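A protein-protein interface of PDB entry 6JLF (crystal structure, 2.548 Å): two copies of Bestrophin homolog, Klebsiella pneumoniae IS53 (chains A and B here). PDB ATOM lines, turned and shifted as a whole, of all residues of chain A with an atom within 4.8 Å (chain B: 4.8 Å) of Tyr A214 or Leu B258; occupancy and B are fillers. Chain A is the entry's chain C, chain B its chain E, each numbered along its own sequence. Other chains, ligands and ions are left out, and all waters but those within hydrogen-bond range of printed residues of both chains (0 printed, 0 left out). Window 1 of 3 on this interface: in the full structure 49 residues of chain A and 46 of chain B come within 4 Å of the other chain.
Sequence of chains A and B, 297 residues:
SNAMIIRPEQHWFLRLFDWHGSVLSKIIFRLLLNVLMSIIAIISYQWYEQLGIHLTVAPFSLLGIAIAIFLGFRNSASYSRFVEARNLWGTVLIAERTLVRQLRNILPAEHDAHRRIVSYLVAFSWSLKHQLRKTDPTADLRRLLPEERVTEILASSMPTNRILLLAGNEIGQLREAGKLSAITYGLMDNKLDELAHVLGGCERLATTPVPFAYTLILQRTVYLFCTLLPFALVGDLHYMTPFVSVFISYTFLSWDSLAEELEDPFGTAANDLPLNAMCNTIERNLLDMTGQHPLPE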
ATOM      1  N   PRO A 211     -23.437   5.077 -30.786  1.00  0.00           N
ATOM      2  CA  PRO A 211     -22.154   4.743 -30.158  1.00  0.00           C
ATOM      3  C   PRO A 211     -22.079   3.244 -29.831  1.00  0.00           C
ATOM      4  O   PRO A 211     -23.075   2.722 -29.364  1.00  0.00           O
ATOM      5  CB  PRO A 211     -22.339   5.500 -28.840  1.00  0.00           C
ATOM      6  CG  PRO A 211     -23.796   5.246 -28.483  1.00  0.00           C
ATOM      7  CD  PRO A 211     -24.513   4.998 -29.799  1.00  0.00           C
ATOM      8  N   PHE A 212     -20.936   2.583 -30.072  1.00  0.00           N
ATOM      9  CA  PHE A 212     -20.890   1.152 -29.777  1.00  0.00           C
ATOM     10  C   PHE A 212     -19.593   0.782 -29.073  1.00  0.00           C
ATOM     11  O   PHE A 212     -18.565   1.419 -29.292  1.00  0.00           O
ATOM     12  CB  PHE A 212     -21.089   0.267 -31.048  1.00  0.00           C
ATOM     13  CG  PHE A 212     -20.553   0.859 -32.342  1.00  0.00           C
ATOM     14  CD1 PHE A 212     -19.178   0.884 -32.610  1.00  0.00           C
ATOM     15  CD2 PHE A 212     -21.417   1.339 -33.320  1.00  0.00           C
ATOM     16  CE1 PHE A 212     -18.675   1.405 -33.833  1.00  0.00           C
ATOM     17  CE2 PHE A 212     -20.923   1.860 -34.522  1.00  0.00           C
ATOM     18  CZ  PHE A 212     -19.552   1.890 -34.779  1.00  0.00           C
ATOM     19  N   ALA A 213     -19.650  -0.262 -28.238  1.00  0.00           N
ATOM     20  CA  ALA A 213     -18.649  -0.697 -27.262  1.00  0.00           C
ATOM     21  C   ALA A 213     -18.289   0.380 -26.255  1.00  0.00           C
ATOM     22  O   ALA A 213     -17.388   0.173 -25.438  1.00  0.00           O
ATOM     23  CB  ALA A 213     -17.395  -1.221 -27.953  1.00  0.00           C
ATOM     24  N   TYR A 214     -18.952   1.536 -26.323  1.00  0.00           N
ATOM     25  CA  TYR A 214     -18.942   2.493 -25.229  1.00  0.00           C
ATOM     26  C   TYR A 214     -20.053   2.214 -24.236  1.00  0.00           C
ATOM     27  O   TYR A 214     -19.890   2.485 -23.042  1.00  0.00           O
ATOM     28  CB  TYR A 214     -19.089   3.924 -25.754  1.00  0.00           C
ATOM     29  CG  TYR A 214     -17.788   4.688 -25.834  1.00  0.00           C
ATOM     30  CD1 TYR A 214     -16.917   4.481 -26.898  1.00  0.00           C
ATOM     31  CD2 TYR A 214     -17.432   5.621 -24.852  1.00  0.00           C
ATOM     32  CE1 TYR A 214     -15.732   5.180 -26.995  1.00  0.00           C
ATOM     33  CE2 TYR A 214     -16.234   6.330 -24.932  1.00  0.00           C
ATOM     34  CZ  TYR A 214     -15.389   6.099 -26.010  1.00  0.00           C
ATOM     35  OH  TYR A 214     -14.203   6.791 -26.115  1.00  0.00           O
ATOM     36  N   THR A 215     -21.183   1.692 -24.710  1.00  0.00           N
ATOM     37  CA  THR A 215     -22.211   1.199 -23.803  1.00  0.00           C
ATOM     38  C   THR A 215     -21.664   0.099 -22.917  1.00  0.00           C
ATOM     39  O   THR A 215     -22.112  -0.067 -21.780  1.00  0.00           O
ATOM     40  CB  THR A 215     -23.383   0.672 -24.610  1.00  0.00           C
ATOM     41  OG1 THR A 215     -22.857   0.044 -25.791  1.00  0.00           O
ATOM     42  CG2 THR A 215     -24.330   1.809 -24.999  1.00  0.00           C
ATOM     43  N   LEU A 216     -20.721  -0.677 -23.447  1.00  0.00           N
ATOM     44  CA  LEU A 216     -19.951  -1.612 -22.640  1.00  0.00           C
ATOM     45  C   LEU A 216     -19.208  -0.884 -21.532  1.00  0.00           C
ATOM     46  O   LEU A 216     -19.254  -1.284 -20.367  1.00  0.00           O
ATOM     47  CB  LEU A 216     -18.968  -2.353 -23.540  1.00  0.00           C
ATOM     48  CG  LEU A 216     -18.559  -3.776 -23.212  1.00  0.00           C
ATOM     49  CD1 LEU A 216     -19.594  -4.741 -23.752  1.00  0.00           C
ATOM     50  CD2 LEU A 216     -17.200  -4.044 -23.830  1.00  0.00           C
ATOM     51  N   ILE A 217     -18.500   0.181 -21.883  1.00  0.00           N
ATOM     52  CA  ILE A 217     -17.865   1.004 -20.868  1.00  0.00           C
ATOM     53  C   ILE A 217     -18.917   1.667 -19.998  1.00  0.00           C
ATOM     54  O   ILE A 217     -18.914   1.530 -18.771  1.00  0.00           O
ATOM     55  CB  ILE A 217     -16.961   2.054 -21.528  1.00  0.00           C
ATOM     56  CG1 ILE A 217     -15.673   1.407 -22.061  1.00  0.00           C
ATOM     57  CG2 ILE A 217     -16.726   3.218 -20.558  1.00  0.00           C
ATOM     58  CD1 ILE A 217     -14.915   2.268 -23.042  1.00  0.00           C
ATOM     59  N   LEU A 218     -19.854   2.375 -20.625  1.00  0.00           N
ATOM     60  CA  LEU A 218     -20.792   3.198 -19.876  1.00  0.00           C
ATOM     61  C   LEU A 218     -21.662   2.379 -18.950  1.00  0.00           C
ATOM     62  O   LEU A 218     -22.267   2.944 -18.029  1.00  0.00           O
ATOM     63  CB  LEU A 218     -21.679   4.029 -20.800  1.00  0.00           C
ATOM     64  CG  LEU A 218     -21.031   5.071 -21.723  1.00  0.00           C
ATOM     65  CD1 LEU A 218     -21.677   5.064 -23.122  1.00  0.00           C
ATOM     66  CD2 LEU A 218     -21.025   6.449 -21.033  1.00  0.00           C
ATOM     67  N   GLN A 219     -21.754   1.070 -19.163  1.00  0.00           N
ATOM     68  CA  GLN A 219     -22.487   0.269 -18.202  1.00  0.00           C
ATOM     69  C   GLN A 219     -21.590  -0.605 -17.339  1.00  0.00           C
ATOM     70  O   GLN A 219     -22.001  -0.964 -16.237  1.00  0.00           O
ATOM     71  CB  GLN A 219     -23.560  -0.570 -18.907  1.00  0.00           C
ATOM     72  CG  GLN A 219     -23.155  -1.937 -19.408  1.00  0.00           C
ATOM     73  CD  GLN A 219     -24.283  -2.593 -20.215  1.00  0.00           C
ATOM     74  OE1 GLN A 219     -25.368  -2.011 -20.382  1.00  0.00           O
ATOM     75  NE2 GLN A 219     -24.024  -3.797 -20.731  1.00  0.00           N
ATOM     76  N   ASN B  75     -22.081  16.654 -24.674  1.00  0.00           N
ATOM     77  CA  ASN B  75     -22.246  15.362 -25.340  1.00  0.00           C
ATOM     78  C   ASN B  75     -23.610  15.230 -26.002  1.00  0.00           C
ATOM     79  O   ASN B  75     -23.766  14.509 -26.986  1.00  0.00           O
ATOM     80  CB  ASN B  75     -22.106  14.241 -24.329  1.00  0.00           C
ATOM     81  CG  ASN B  75     -20.693  13.905 -24.017  1.00  0.00           C
ATOM     82  OD1 ASN B  75     -19.827  14.770 -23.986  1.00  0.00           O
ATOM     83  ND2 ASN B  75     -20.448  12.627 -23.747  1.00  0.00           N
ATOM     84  N   LEU B 253     -13.591  10.727 -18.095  1.00  0.00           N
ATOM     85  CA  LEU B 253     -12.840  10.790 -19.341  1.00  0.00           C
ATOM     86  C   LEU B 253     -13.487   9.937 -20.415  1.00  0.00           C
ATOM     87  O   LEU B 253     -13.513  10.338 -21.582  1.00  0.00           O
ATOM     88  CB  LEU B 253     -11.397  10.350 -19.108  1.00  0.00           C
ATOM     89  CG  LEU B 253     -10.535  11.297 -18.272  1.00  0.00           C
ATOM     90  CD1 LEU B 253      -9.174  10.677 -18.049  1.00  0.00           C
ATOM     91  CD2 LEU B 253     -10.414  12.618 -18.949  1.00  0.00           C
ATOM     92  N   SER B 254     -13.995   8.761 -20.034  1.00  0.00           N
ATOM     93  CA  SER B 254     -14.939   8.023 -20.870  1.00  0.00           C
ATOM     94  C   SER B 254     -16.033   8.924 -21.426  1.00  0.00           C
ATOM     95  O   SER B 254     -16.280   8.941 -22.638  1.00  0.00           O
ATOM     96  CB  SER B 254     -15.587   6.897 -20.073  1.00  0.00           C
ATOM     97  OG  SER B 254     -14.674   5.844 -19.866  1.00  0.00           O
ATOM     98  N   TRP B 255     -16.729   9.651 -20.546  1.00  0.00           N
ATOM     99  CA  TRP B 255     -17.835  10.479 -21.006  1.00  0.00           C
ATOM    100  C   TRP B 255     -17.332  11.616 -21.869  1.00  0.00           C
ATOM    101  O   TRP B 255     -17.974  11.984 -22.856  1.00  0.00           O
ATOM    102  CB  TRP B 255     -18.642  11.032 -19.825  1.00  0.00           C
ATOM    103  CG  TRP B 255     -19.909  11.735 -20.251  1.00  0.00           C
ATOM    104  CD1 TRP B 255     -20.100  13.089 -20.371  1.00  0.00           C
ATOM    105  CD2 TRP B 255     -21.167  11.120 -20.614  1.00  0.00           C
ATOM    106  NE1 TRP B 255     -21.402  13.354 -20.779  1.00  0.00           N
ATOM    107  CE2 TRP B 255     -22.072  12.167 -20.940  1.00  0.00           C
ATOM    108  CE3 TRP B 255     -21.617   9.791 -20.684  1.00  0.00           C
ATOM    109  CZ2 TRP B 255     -23.400  11.926 -21.332  1.00  0.00           C
ATOM    110  CZ3 TRP B 255     -22.943   9.551 -21.068  1.00  0.00           C
ATOM    111  CH2 TRP B 255     -23.817  10.617 -21.390  1.00  0.00           C
ATOM    112  N   ASP B 256     -16.197  12.201 -21.512  1.00  0.00           N
ATOM    113  CA  ASP B 256     -15.717  13.317 -22.312  1.00  0.00           C
ATOM    114  C   ASP B 256     -15.215  12.844 -23.669  1.00  0.00           C
ATOM    115  O   ASP B 256     -15.386  13.539 -24.679  1.00  0.00           O
ATOM    116  CB  ASP B 256     -14.631  14.071 -21.564  1.00  0.00           C
ATOM    117  CG  ASP B 256     -13.980  15.112 -22.412  1.00  0.00           C
ATOM    118  OD1 ASP B 256     -14.706  15.948 -22.985  1.00  0.00           O
ATOM    119  OD2 ASP B 256     -12.732  15.102 -22.505  1.00  0.00           O
ATOM    120  N   SER B 257     -14.627  11.656 -23.719  1.00  0.00           N
ATOM    121  CA  SER B 257     -14.086  11.153 -24.969  1.00  0.00           C
ATOM    122  C   SER B 257     -15.175  10.591 -25.875  1.00  0.00           C
ATOM    123  O   SER B 257     -14.929  10.367 -27.061  1.00  0.00           O
ATOM    124  CB  SER B 257     -13.027  10.079 -24.689  1.00  0.00           C
ATOM    125  OG  SER B 257     -13.636   8.807 -24.672  1.00  0.00           O
ATOM    126  N   LEU B 258     -16.350  10.297 -25.327  1.00  0.00           N
ATOM    127  CA  LEU B 258     -17.476   9.921 -26.164  1.00  0.00           C
ATOM    128  C   LEU B 258     -17.853  11.060 -27.094  1.00  0.00           C
ATOM    129  O   LEU B 258     -18.143  10.842 -28.274  1.00  0.00           O
ATOM    130  CB  LEU B 258     -18.652   9.527 -25.293  1.00  0.00           C
ATOM    131  CG  LEU B 258     -19.882   9.113 -26.083  1.00  0.00           C
ATOM    132  CD1 LEU B 258     -19.530   7.915 -26.932  1.00  0.00           C
ATOM    133  CD2 LEU B 258     -21.027   8.815 -25.121  1.00  0.00           C
ATOM    134  N   ALA B 259     -17.819  12.289 -26.588  1.00  0.00           N
ATOM    135  CA  ALA B 259     -18.066  13.432 -27.454  1.00  0.00           C
ATOM    136  C   ALA B 259     -17.065  13.480 -28.588  1.00  0.00           C
ATOM    137  O   ALA B 259     -17.429  13.801 -29.716  1.00  0.00           O
ATOM    138  CB  ALA B 259     -18.012  14.738 -26.664  1.00  0.00           C
ATOM    139  N   GLU B 260     -15.814  13.129 -28.332  1.00  0.00           N
ATOM    140  CA  GLU B 260     -14.850  13.203 -29.415  1.00  0.00           C
ATOM    141  C   GLU B 260     -15.026  12.053 -30.405  1.00  0.00           C
ATOM    142  O   GLU B 260     -14.782  12.239 -31.598  1.00  0.00           O
ATOM    143  CB  GLU B 260     -13.425  13.280 -28.844  1.00  0.00           C
ATOM    144  CG  GLU B 260     -12.300  13.559 -29.903  1.00  0.00           C
ATOM    145  CD  GLU B 260     -11.885  15.067 -30.028  1.00  0.00           C
ATOM    146  OE1 GLU B 260     -11.774  15.769 -28.991  1.00  0.00           O
ATOM    147  OE2 GLU B 260     -11.670  15.542 -31.176  1.00  0.00           O
ATOM    148  N   GLU B 261     -15.536  10.907 -29.972  1.00  0.00           N
ATOM    149  CA  GLU B 261     -15.872   9.852 -30.929  1.00  0.00           C
ATOM    150  C   GLU B 261     -17.028  10.230 -31.866  1.00  0.00           C
ATOM    151  O   GLU B 261     -17.222   9.571 -32.894  1.00  0.00           O
ATOM    152  CB  GLU B 261     -16.244   8.566 -30.198  1.00  0.00           C
ATOM    153  CG  GLU B 261     -15.153   7.993 -29.392  1.00  0.00           C
ATOM    154  CD  GLU B 261     -14.531   6.825 -30.091  1.00  0.00           C
ATOM    155  OE1 GLU B 261     -13.476   7.006 -30.737  1.00  0.00           O
ATOM    156  OE2 GLU B 261     -15.119   5.725 -30.027  1.00  0.00           O
ATOM    157  N   LEU B 262     -17.823  11.239 -31.520  1.00  0.00           N
ATOM    158  CA  LEU B 262     -19.004  11.612 -32.269  1.00  0.00           C
ATOM    159  C   LEU B 262     -18.819  12.912 -33.050  1.00  0.00           C
ATOM    160  O   LEU B 262     -19.753  13.360 -33.741  1.00  0.00           O
ATOM    161  CB  LEU B 262     -20.196  11.727 -31.321  1.00  0.00           C
ATOM    162  CG  LEU B 262     -20.645  10.427 -30.601  1.00  0.00           C
ATOM    163  CD1 LEU B 262     -21.728  10.776 -29.661  1.00  0.00           C
ATOM    164  CD2 LEU B 262     -21.105   9.264 -31.501  1.00  0.00           C
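OH of Tyr A214 sits at hydrogen-bond distance from OG of Ser B257 (2.5 Å).
ND2 of Asn B75 lies within hydrogen-bond range of O of Trp B255, 2.7 Å away. The side-chain hydroxyl (OG) of Ser B257 lies close to the backbone carbonyl oxygen (O) of Leu B253 (3.5 Å). The side-chain hydroxyl (OG) of Ser B257 is in hydrogen-bond range of the backbone carbonyl oxygen (O) of Ser B254 (3.3 Å).
Among the printed residues, merely in contact across the chains: Tyr A214 with Glu B261 (3.1 Å), Ile A217 with Ser B254 (3.4 Å), Leu A218 with Trp B255 (3.4 Å), Tyr A214 with Ser B254 (3.5 Å) and Tyr A214 with Leu B258 (3.7 Å).
Of chain B, only Ser B254, Ser B257, Leu B258 and Glu B261 come within 4 Å of Tyr A214. Of chain A, only Tyr A214 (3.7 Å) comes within 4 Å of Leu B258. Of the printed residues of chain A, Glu B261 touches Tyr A214. Of the printed residues of chain B, Leu A218 touches Trp B255. Printed residues of chain A within 4 Å of Trp B255: Leu A218. Of the printed residues of chain B, Ile A217 touches Ser B254 (3.4 Å). Of the printed residues of chain A, Ser B257 touches Tyr A214 (2.5 Å). Ala B259 touches none of the printed residues of chain A. Leu A216 touches none of the printed residues of chain B. The nearest residue of chain A that does not touch Leu B258 is Pro A211 (4.2 Å).
Of the 11 printed residues of chain B, 5 touch a printed residue of chain A. Printed residues of chain B that touch a printed residue of chain A: Ser B254, Trp B255, Ser B257, Leu B258 and Glu B261. Hydrophobic or aromatic side chains of chain B within 4 Å of the printed part of chain A: Trp B255 and Leu B258. Of the 9 printed residues of chain A, 3 touch a printed residue of chain B. Hydrophobic or aromatic side chains of chain A within 4 Å of the printed part of chain B: Tyr A214, Ile A217 and Leu A218. Among the printed residues, no Asp or Glu carboxylate lies within 4 Å of a Lys or Arg side-chain nitrogen of the other chain.
No position is printed for both chains.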
